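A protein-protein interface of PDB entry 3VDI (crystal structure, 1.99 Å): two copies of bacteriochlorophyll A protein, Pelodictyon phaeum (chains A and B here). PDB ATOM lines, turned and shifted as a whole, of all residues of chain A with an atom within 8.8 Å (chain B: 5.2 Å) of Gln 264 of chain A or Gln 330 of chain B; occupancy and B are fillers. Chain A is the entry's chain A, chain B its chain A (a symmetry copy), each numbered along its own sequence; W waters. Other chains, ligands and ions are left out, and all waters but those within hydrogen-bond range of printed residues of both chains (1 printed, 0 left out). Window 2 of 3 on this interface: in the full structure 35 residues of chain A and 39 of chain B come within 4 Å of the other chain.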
ATOM      1  N   THR A  10     -18.051 -23.519   3.979  1.00  0.00           N
ATOM      2  CA  THR A  10     -19.187 -22.654   3.658  1.00  0.00           C
ATOM      3  C   THR A  10     -20.471 -23.386   4.004  1.00  0.00           C
ATOM      4  O   THR A  10     -20.734 -24.482   3.502  1.00  0.00           O
ATOM      5  CB  THR A  10     -19.144 -22.167   2.225  1.00  0.00           C
ATOM      6  OG1 THR A  10     -17.830 -21.703   1.895  1.00  0.00           O
ATOM      7  CG2 THR A  10     -20.190 -21.112   1.956  1.00  0.00           C
ATOM      8  N   THR A  11     -21.247 -22.802   4.911  1.00  0.00           N
ATOM      9  CA  THR A  11     -22.461 -23.451   5.391  1.00  0.00           C
ATOM     10  C   THR A  11     -23.620 -22.504   5.425  1.00  0.00           C
ATOM     11  O   THR A  11     -23.481 -21.370   5.876  1.00  0.00           O
ATOM     12  CB  THR A  11     -22.200 -24.099   6.777  1.00  0.00           C
ATOM     13  OG1 THR A  11     -21.075 -24.966   6.662  1.00  0.00           O
ATOM     14  CG2 THR A  11     -23.384 -24.923   7.289  1.00  0.00           C
ATOM     15  N   LYS A  35     -28.601 -17.853   7.826  1.00  0.00           N
ATOM     16  CA  LYS A  35     -27.304 -17.218   7.918  1.00  0.00           C
ATOM     17  C   LYS A  35     -26.338 -18.038   7.087  1.00  0.00           C
ATOM     18  O   LYS A  35     -26.366 -19.275   7.135  1.00  0.00           O
ATOM     19  CB  LYS A  35     -26.823 -17.008   9.375  1.00  0.00           C
ATOM     20  CG  LYS A  35     -26.406 -18.241  10.166  1.00  0.00           C
ATOM     21  CD  LYS A  35     -25.904 -17.870  11.568  1.00  0.00           C
ATOM     22  CE  LYS A  35     -24.497 -17.302  11.599  1.00  0.00           C
ATOM     23  NZ  LYS A  35     -24.059 -16.972  12.988  1.00  0.00           N
ATOM     24  N   VAL A  36     -25.535 -17.347   6.275  1.00  0.00           N
ATOM     25  CA  VAL A  36     -24.561 -17.976   5.391  1.00  0.00           C
ATOM     26  C   VAL A  36     -23.335 -17.085   5.323  1.00  0.00           C
ATOM     27  O   VAL A  36     -23.454 -15.860   5.180  1.00  0.00           O
ATOM     28  CB  VAL A  36     -25.172 -18.323   4.004  1.00  0.00           C
ATOM     29  CG1 VAL A  36     -25.710 -17.086   3.295  1.00  0.00           C
ATOM     30  CG2 VAL A  36     -24.190 -19.094   3.116  1.00  0.00           C
ATOM     31  N   ASN A  37     -22.156 -17.709   5.459  1.00  0.00           N
ATOM     32  CA  ASN A  37     -20.880 -17.020   5.491  1.00  0.00           C
ATOM     33  C   ASN A  37     -20.312 -16.819   4.087  1.00  0.00           C
ATOM     34  O   ASN A  37     -19.214 -17.274   3.791  1.00  0.00           O
ATOM     35  CB  ASN A  37     -19.904 -17.766   6.416  1.00  0.00           C
ATOM     36  CG  ASN A  37     -19.573 -19.193   5.985  1.00  0.00           C
ATOM     37  OD1 ASN A  37     -20.391 -19.921   5.404  1.00  0.00           O
ATOM     38  ND2 ASN A  37     -18.331 -19.590   6.180  1.00  0.00           N
ATOM     39  N   VAL A  38     -21.084 -16.158   3.222  1.00  0.00           N
ATOM     40  CA  VAL A  38     -20.701 -15.820   1.838  1.00  0.00           C
ATOM     41  C   VAL A  38     -20.913 -14.322   1.615  1.00  0.00           C
ATOM     42  O   VAL A  38     -21.795 -13.745   2.256  1.00  0.00           O
ATOM     43  CB  VAL A  38     -21.471 -16.651   0.752  1.00  0.00           C
ATOM     44  CG1 VAL A  38     -21.197 -18.148   0.896  1.00  0.00           C
ATOM     45  CG2 VAL A  38     -22.977 -16.360   0.736  1.00  0.00           C
ATOM     46  N   PRO A  39     -20.195 -13.670   0.685  1.00  0.00           N
ATOM     47  CA  PRO A  39     -20.544 -12.274   0.384  1.00  0.00           C
ATOM     48  C   PRO A  39     -21.898 -12.200  -0.332  1.00  0.00           C
ATOM     49  O   PRO A  39     -22.262 -13.121  -1.068  1.00  0.00           O
ATOM     50  CB  PRO A  39     -19.446 -11.835  -0.602  1.00  0.00           C
ATOM     51  CG  PRO A  39     -18.933 -13.094  -1.202  1.00  0.00           C
ATOM     52  CD  PRO A  39     -19.123 -14.183  -0.203  1.00  0.00           C
ATOM     53  N   ALA A  40     -22.611 -11.071  -0.172  1.00  0.00           N
ATOM     54  CA  ALA A  40     -23.803 -10.749  -0.977  1.00  0.00           C
ATOM     55  C   ALA A  40     -23.192 -10.325  -2.344  1.00  0.00           C
ATOM     56  O   ALA A  40     -21.991 -10.035  -2.401  1.00  0.00           O
ATOM     57  CB  ALA A  40     -24.557  -9.579  -0.361  1.00  0.00           C
ATOM     58  N   LEU A  45     -21.452  -2.464  -0.598  1.00  0.00           N
ATOM     59  CA  LEU A  45     -21.645  -3.116   0.698  1.00  0.00           C
ATOM     60  C   LEU A  45     -21.021  -2.294   1.845  1.00  0.00           C
ATOM     61  O   LEU A  45     -20.146  -1.486   1.577  1.00  0.00           O
ATOM     62  CB  LEU A  45     -21.009  -4.547   0.667  1.00  0.00           C
ATOM     63  CG  LEU A  45     -21.697  -5.576  -0.247  1.00  0.00           C
ATOM     64  CD1 LEU A  45     -20.788  -6.798  -0.461  1.00  0.00           C
ATOM     65  CD2 LEU A  45     -23.071  -5.981   0.300  1.00  0.00           C
ATOM     66  N   PRO A  46     -21.366  -2.519   3.133  1.00  0.00           N
ATOM     67  CA  PRO A  46     -22.399  -3.438   3.652  1.00  0.00           C
ATOM     68  C   PRO A  46     -23.795  -2.958   3.284  1.00  0.00           C
ATOM     69  O   PRO A  46     -23.977  -1.814   2.848  1.00  0.00           O
ATOM     70  CB  PRO A  46     -22.176  -3.402   5.175  1.00  0.00           C
ATOM     71  CG  PRO A  46     -21.536  -2.083   5.444  1.00  0.00           C
ATOM     72  CD  PRO A  46     -20.702  -1.773   4.227  1.00  0.00           C
ATOM     73  N   ARG A 260     -29.057  -8.424   7.074  1.00  0.00           N
ATOM     74  CA  ARG A 260     -27.784  -7.746   7.318  1.00  0.00           C
ATOM     75  C   ARG A 260     -26.784  -8.452   6.442  1.00  0.00           C
ATOM     76  O   ARG A 260     -26.686  -9.683   6.489  1.00  0.00           O
ATOM     77  CB  ARG A 260     -27.332  -7.845   8.798  1.00  0.00           C
ATOM     78  CG  ARG A 260     -28.332  -7.247   9.795  1.00  0.00           C
ATOM     79  CD  ARG A 260     -27.688  -7.000  11.143  1.00  0.00           C
ATOM     80  NE  ARG A 260     -27.013  -5.704  11.141  1.00  0.00           N
ATOM     81  CZ  ARG A 260     -25.701  -5.530  11.249  1.00  0.00           C
ATOM     82  NH1 ARG A 260     -24.893  -6.576  11.412  1.00  0.00           N
ATOM     83  NH2 ARG A 260     -25.184  -4.309  11.205  1.00  0.00           N
ATOM     84  N   SER A 261     -26.055  -7.704   5.627  1.00  0.00           N
ATOM     85  CA  SER A 261     -25.098  -8.350   4.741  1.00  0.00           C
ATOM     86  C   SER A 261     -23.835  -7.518   4.552  1.00  0.00           C
ATOM     87  O   SER A 261     -23.858  -6.306   4.704  1.00  0.00           O
ATOM     88  CB  SER A 261     -25.753  -8.602   3.380  1.00  0.00           C
ATOM     89  OG  SER A 261     -25.910  -7.408   2.621  1.00  0.00           O
ATOM     90  N   ASP A 262     -22.751  -8.177   4.160  1.00  0.00           N
ATOM     91  CA  ASP A 262     -21.484  -7.544   3.831  1.00  0.00           C
ATOM     92  C   ASP A 262     -20.705  -8.522   2.955  1.00  0.00           C
ATOM     93  O   ASP A 262     -21.279  -9.539   2.551  1.00  0.00           O
ATOM     94  CB  ASP A 262     -20.731  -7.055   5.091  1.00  0.00           C
ATOM     95  CG  ASP A 262     -20.222  -8.118   6.048  1.00  0.00           C
ATOM     96  OD1 ASP A 262     -20.292  -9.318   5.705  1.00  0.00           O
ATOM     97  OD2 ASP A 262     -19.680  -7.747   7.102  1.00  0.00           O
ATOM     98  N   SER A 263     -19.413  -8.279   2.730  1.00  0.00           N
ATOM     99  CA  SER A 263     -18.578  -9.120   1.877  1.00  0.00           C
ATOM    100  C   SER A 263     -18.169 -10.469   2.529  1.00  0.00           C
ATOM    101  O   SER A 263     -17.420 -11.245   1.932  1.00  0.00           O
ATOM    102  CB  SER A 263     -17.347  -8.342   1.423  1.00  0.00           C
ATOM    103  OG  SER A 263     -16.578  -8.016   2.571  1.00  0.00           O
ATOM    104  N   GLN A 264     -18.658 -10.742   3.718  1.00  0.00           N
ATOM    105  CA  GLN A 264     -18.325 -11.988   4.397  1.00  0.00           C
ATOM    106  C   GLN A 264     -19.541 -12.762   4.883  1.00  0.00           C
ATOM    107  O   GLN A 264     -19.376 -13.889   5.310  1.00  0.00           O
ATOM    108  CB  GLN A 264     -17.356 -11.719   5.577  1.00  0.00           C
ATOM    109  CG  GLN A 264     -15.930 -11.458   5.144  1.00  0.00           C
ATOM    110  CD  GLN A 264     -15.384 -10.085   5.449  1.00  0.00           C
ATOM    111  OE1 GLN A 264     -15.923  -9.057   5.002  1.00  0.00           O
ATOM    112  NE2 GLN A 264     -14.217 -10.054   6.119  1.00  0.00           N
ATOM    113  N   GLY A 265     -20.748 -12.177   4.827  1.00  0.00           N
ATOM    114  CA  GLY A 265     -21.905 -12.899   5.347  1.00  0.00           C
ATOM    115  C   GLY A 265     -23.246 -12.280   5.042  1.00  0.00           C
ATOM    116  O   GLY A 265     -23.332 -11.104   4.677  1.00  0.00           O
ATOM    117  N   ILE A 266     -24.299 -13.104   5.155  1.00  0.00           N
ATOM    118  CA  ILE A 266     -25.681 -12.673   4.941  1.00  0.00           C
ATOM    119  C   ILE A 266     -26.472 -13.283   6.073  1.00  0.00           C
ATOM    120  O   ILE A 266     -26.274 -14.447   6.391  1.00  0.00           O
ATOM    121  CB  ILE A 266     -26.264 -13.108   3.550  1.00  0.00           C
ATOM    122  CG1 ILE A 266     -25.367 -12.686   2.364  1.00  0.00           C
ATOM    123  CG2 ILE A 266     -27.725 -12.592   3.373  1.00  0.00           C
ATOM    124  CD1 ILE A 266     -25.706 -13.377   1.010  1.00  0.00           C
ATOM    125  N   GLU A 267     -27.337 -12.500   6.710  1.00  0.00           N
ATOM    126  CA  GLU A 267     -28.213 -13.032   7.752  1.00  0.00           C
ATOM    127  C   GLU A 267     -29.584 -12.411   7.568  1.00  0.00           C
ATOM    128  O   GLU A 267     -29.693 -11.226   7.257  1.00  0.00           O
ATOM    129  CB  GLU A 267     -27.652 -12.843   9.178  1.00  0.00           C
ATOM    130  CG  GLU A 267     -27.703 -11.406   9.675  1.00  0.00           C
ATOM    131  CD  GLU A 267     -27.280 -11.188  11.114  1.00  0.00           C
ATOM    132  OE1 GLU A 267     -27.945 -10.386  11.810  1.00  0.00           O
ATOM    133  OE2 GLU A 267     -26.290 -11.822  11.547  1.00  0.00           O
ATOM    134  N   ASN A 306     -21.298 -19.407  -4.550  1.00  0.00           N
ATOM    135  CA  ASN A 306     -20.385 -20.090  -3.634  1.00  0.00           C
ATOM    136  C   ASN A 306     -20.965 -21.446  -3.273  1.00  0.00           C
ATOM    137  O   ASN A 306     -22.142 -21.541  -2.921  1.00  0.00           O
ATOM    138  CB  ASN A 306     -20.157 -19.298  -2.334  1.00  0.00           C
ATOM    139  CG  ASN A 306     -19.367 -18.024  -2.414  1.00  0.00           C
ATOM    140  OD1 ASN A 306     -19.916 -16.914  -2.436  1.00  0.00           O
ATOM    141  ND2 ASN A 306     -18.058 -18.151  -2.403  1.00  0.00           N
ATOM    142  N   ALA B 327     -10.549  -2.206   4.909  1.00  0.00           N
ATOM    143  CA  ALA B 327     -10.494  -3.301   3.932  1.00  0.00           C
ATOM    144  C   ALA B 327     -11.565  -4.327   4.265  1.00  0.00           C
ATOM    145  O   ALA B 327     -11.604  -4.824   5.400  1.00  0.00           O
ATOM    146  CB  ALA B 327      -9.117  -3.957   3.927  1.00  0.00           C
ATOM    147  N   ALA B 328     -12.466  -4.602   3.290  1.00  0.00           N
ATOM    148  CA  ALA B 328     -13.555  -5.582   3.428  1.00  0.00           C
ATOM    149  C   ALA B 328     -13.799  -6.361   2.104  1.00  0.00           C
ATOM    150  O   ALA B 328     -14.271  -5.753   1.154  1.00  0.00           O
ATOM    151  CB  ALA B 328     -14.840  -4.914   3.918  1.00  0.00           C
ATOM    152  N   PRO B 329     -13.455  -7.676   1.994  1.00  0.00           N
ATOM    153  CA  PRO B 329     -12.868  -8.560   3.035  1.00  0.00           C
ATOM    154  C   PRO B 329     -11.545  -8.035   3.592  1.00  0.00           C
ATOM    155  O   PRO B 329     -10.745  -7.434   2.866  1.00  0.00           O
ATOM    156  CB  PRO B 329     -12.673  -9.896   2.292  1.00  0.00           C
ATOM    157  CG  PRO B 329     -13.722  -9.857   1.208  1.00  0.00           C
ATOM    158  CD  PRO B 329     -13.707  -8.432   0.749  1.00  0.00           C
ATOM    159  N   GLN B 330     -11.340  -8.243   4.900  1.00  0.00           N
ATOM    160  CA  GLN B 330     -10.164  -7.810   5.632  1.00  0.00           C
ATOM    161  C   GLN B 330      -8.946  -8.551   5.117  1.00  0.00           C
ATOM    162  O   GLN B 330      -9.057  -9.713   4.715  1.00  0.00           O
ATOM    163  CB  GLN B 330     -10.338  -8.078   7.139  1.00  0.00           C
ATOM    164  CG  GLN B 330     -11.497  -7.310   7.775  1.00  0.00           C
ATOM    165  CD  GLN B 330     -11.759  -7.731   9.203  1.00  0.00           C
ATOM    166  OE1 GLN B 330     -12.703  -8.475   9.497  1.00  0.00           O
ATOM    167  NE2 GLN B 330     -10.951  -7.236  10.129  1.00  0.00           N
ATOM    168  N   PHE B 331      -7.789  -7.877   5.089  1.00  0.00           N
ATOM    169  CA  PHE B 331      -6.545  -8.536   4.669  1.00  0.00           C
ATOM    170  C   PHE B 331      -6.173  -9.563   5.752  1.00  0.00           C
ATOM    171  O   PHE B 331      -6.583  -9.397   6.909  1.00  0.00           O
ATOM    172  CB  PHE B 331      -5.406  -7.515   4.438  1.00  0.00           C
ATOM    173  CG  PHE B 331      -5.211  -6.508   5.553  1.00  0.00           C
ATOM    174  CD1 PHE B 331      -4.406  -6.805   6.654  1.00  0.00           C
ATOM    175  CD2 PHE B 331      -5.794  -5.245   5.482  1.00  0.00           C
ATOM    176  CE1 PHE B 331      -4.240  -5.880   7.691  1.00  0.00           C
ATOM    177  CE2 PHE B 331      -5.621  -4.315   6.522  1.00  0.00           C
ATOM    178  CZ  PHE B 331      -4.836  -4.636   7.607  1.00  0.00           C
ATOM    179  N   ARG B 332      -5.464 -10.644   5.363  1.00  0.00           N
ATOM    180  CA  ARG B 332      -5.016 -11.700   6.277  1.00  0.00           C
ATOM    181  C   ARG B 332      -3.772 -11.245   7.075  1.00  0.00           C
ATOM    182  O   ARG B 332      -3.721 -11.439   8.288  1.00  0.00           O
ATOM    183  CB  ARG B 332      -4.668 -12.973   5.482  1.00  0.00           C
ATOM    184  CG  ARG B 332      -4.162 -14.134   6.366  1.00  0.00           C
ATOM    185  CD  ARG B 332      -4.067 -15.404   5.577  1.00  0.00           C
ATOM    186  NE  ARG B 332      -4.038 -16.597   6.420  1.00  0.00           N
ATOM    187  CZ  ARG B 332      -4.268 -17.825   5.969  1.00  0.00           C
ATOM    188  NH1 ARG B 332      -4.553 -18.028   4.683  1.00  0.00           N
ATOM    189  NH2 ARG B 332      -4.229 -18.862   6.798  1.00  0.00           N
ATOM    190  N   TRP B 341      -3.955 -10.986   1.106  1.00  0.00           N
ATOM    191  CA  TRP B 341      -5.235 -11.641   1.286  1.00  0.00           C
ATOM    192  C   TRP B 341      -5.072 -13.073   0.793  1.00  0.00           C
ATOM    193  O   TRP B 341      -4.592 -13.284  -0.328  1.00  0.00           O
ATOM    194  CB  TRP B 341      -6.327 -10.972   0.407  1.00  0.00           C
ATOM    195  CG  TRP B 341      -6.860  -9.667   0.920  1.00  0.00           C
ATOM    196  CD1 TRP B 341      -8.095  -9.441   1.454  1.00  0.00           C
ATOM    197  CD2 TRP B 341      -6.252  -8.385   0.755  1.00  0.00           C
ATOM    198  NE1 TRP B 341      -8.272  -8.097   1.683  1.00  0.00           N
ATOM    199  CE2 TRP B 341      -7.152  -7.423   1.272  1.00  0.00           C
ATOM    200  CE3 TRP B 341      -4.995  -7.951   0.277  1.00  0.00           C
ATOM    201  CZ2 TRP B 341      -6.837  -6.061   1.340  1.00  0.00           C
ATOM    202  CZ3 TRP B 341      -4.700  -6.597   0.313  1.00  0.00           C
ATOM    203  CH2 TRP B 341      -5.619  -5.667   0.830  1.00  0.00           C
ATOM    204  N   ALA B 345     -12.420 -15.470   4.160  1.00  0.00           N
ATOM    205  CA  ALA B 345     -13.339 -14.562   3.494  1.00  0.00           C
ATOM    206  C   ALA B 345     -12.900 -14.157   2.070  1.00  0.00           C
ATOM    207  O   ALA B 345     -13.733 -14.116   1.167  1.00  0.00           O
ATOM    208  CB  ALA B 345     -13.538 -13.329   4.361  1.00  0.00           C
HETATM  209  O   HOH W   1     -16.353 -13.750   1.850  1.00  0.00           O
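Among the printed residues, pairs that only touch across the chains: Ser 263 of chain A with Ala 328 of chain B, Gln 264 of chain A with Pro 329 of chain B, Gln 264 of chain A with Gln 330 of chain B and Gln 264 of chain A with Ala 345 of chain B.
OG of Ser 263 of chain A sits close to N of Pro 329 of chain B (3.2 Å).
No position is printed for both chains.
Of the 8 printed residues of chain B, 4 touch a printed residue of chain A. Among the printed residues, 5 pairs touch across the chains.
Water W1 lies within hydrogen-bond range of the backbone carbonyl oxygen (O) of Ser 263 of chain A (2.7 Å) and the backbone carbonyl oxygen (O) of Ala 345 of chain B (2.7 Å).
Gln 264 of chain A touches just these residues of chain B: Pro 329 (3.7 Å), Gln 330 (3.6 Å) and Ala 345 (3.1 Å). Of chain A, only Gln 264 (3.6 Å) comes within 4 Å of Gln 330 of chain B. Of the printed residues of chain B, Ser 263 of chain A touches Ala 328 and Pro 329. Of the printed residues of chain A, Ala 328 of chain B touches Ser 263 (3.3 Å). Pro 46 of chain A touches none of the printed residues of chain B. The nearest residue of chain B that does not touch Gln 264 of chain A is Ala 328 of chain B (4.4 Å). The nearest residue of chain A that does not touch Gln 330 of chain B is Ser 263 of chain A (5.7 Å). The nearest printed residue of chain B that does not touch Ser 263 of chain A is Ala 345 of chain B (4.7 Å).
The side-chain carboxylate (OD1) of Asp 262 of chain A lies within hydrogen-bond range of the backbone NH (N) of Gln 264 of chain A (2.9 Å). The side-chain amide oxygen (OE1) of Gln 264 of chain A lies within hydrogen-bond range of the side-chain hydroxyl (OG) of Ser 263 of chain A (2.7 Å). The backbone carbonyl oxygen of Pro 329 of chain B lies within hydrogen-bond range of the indole nitrogen of Trp 341 of chain B, 2.8 Å away.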
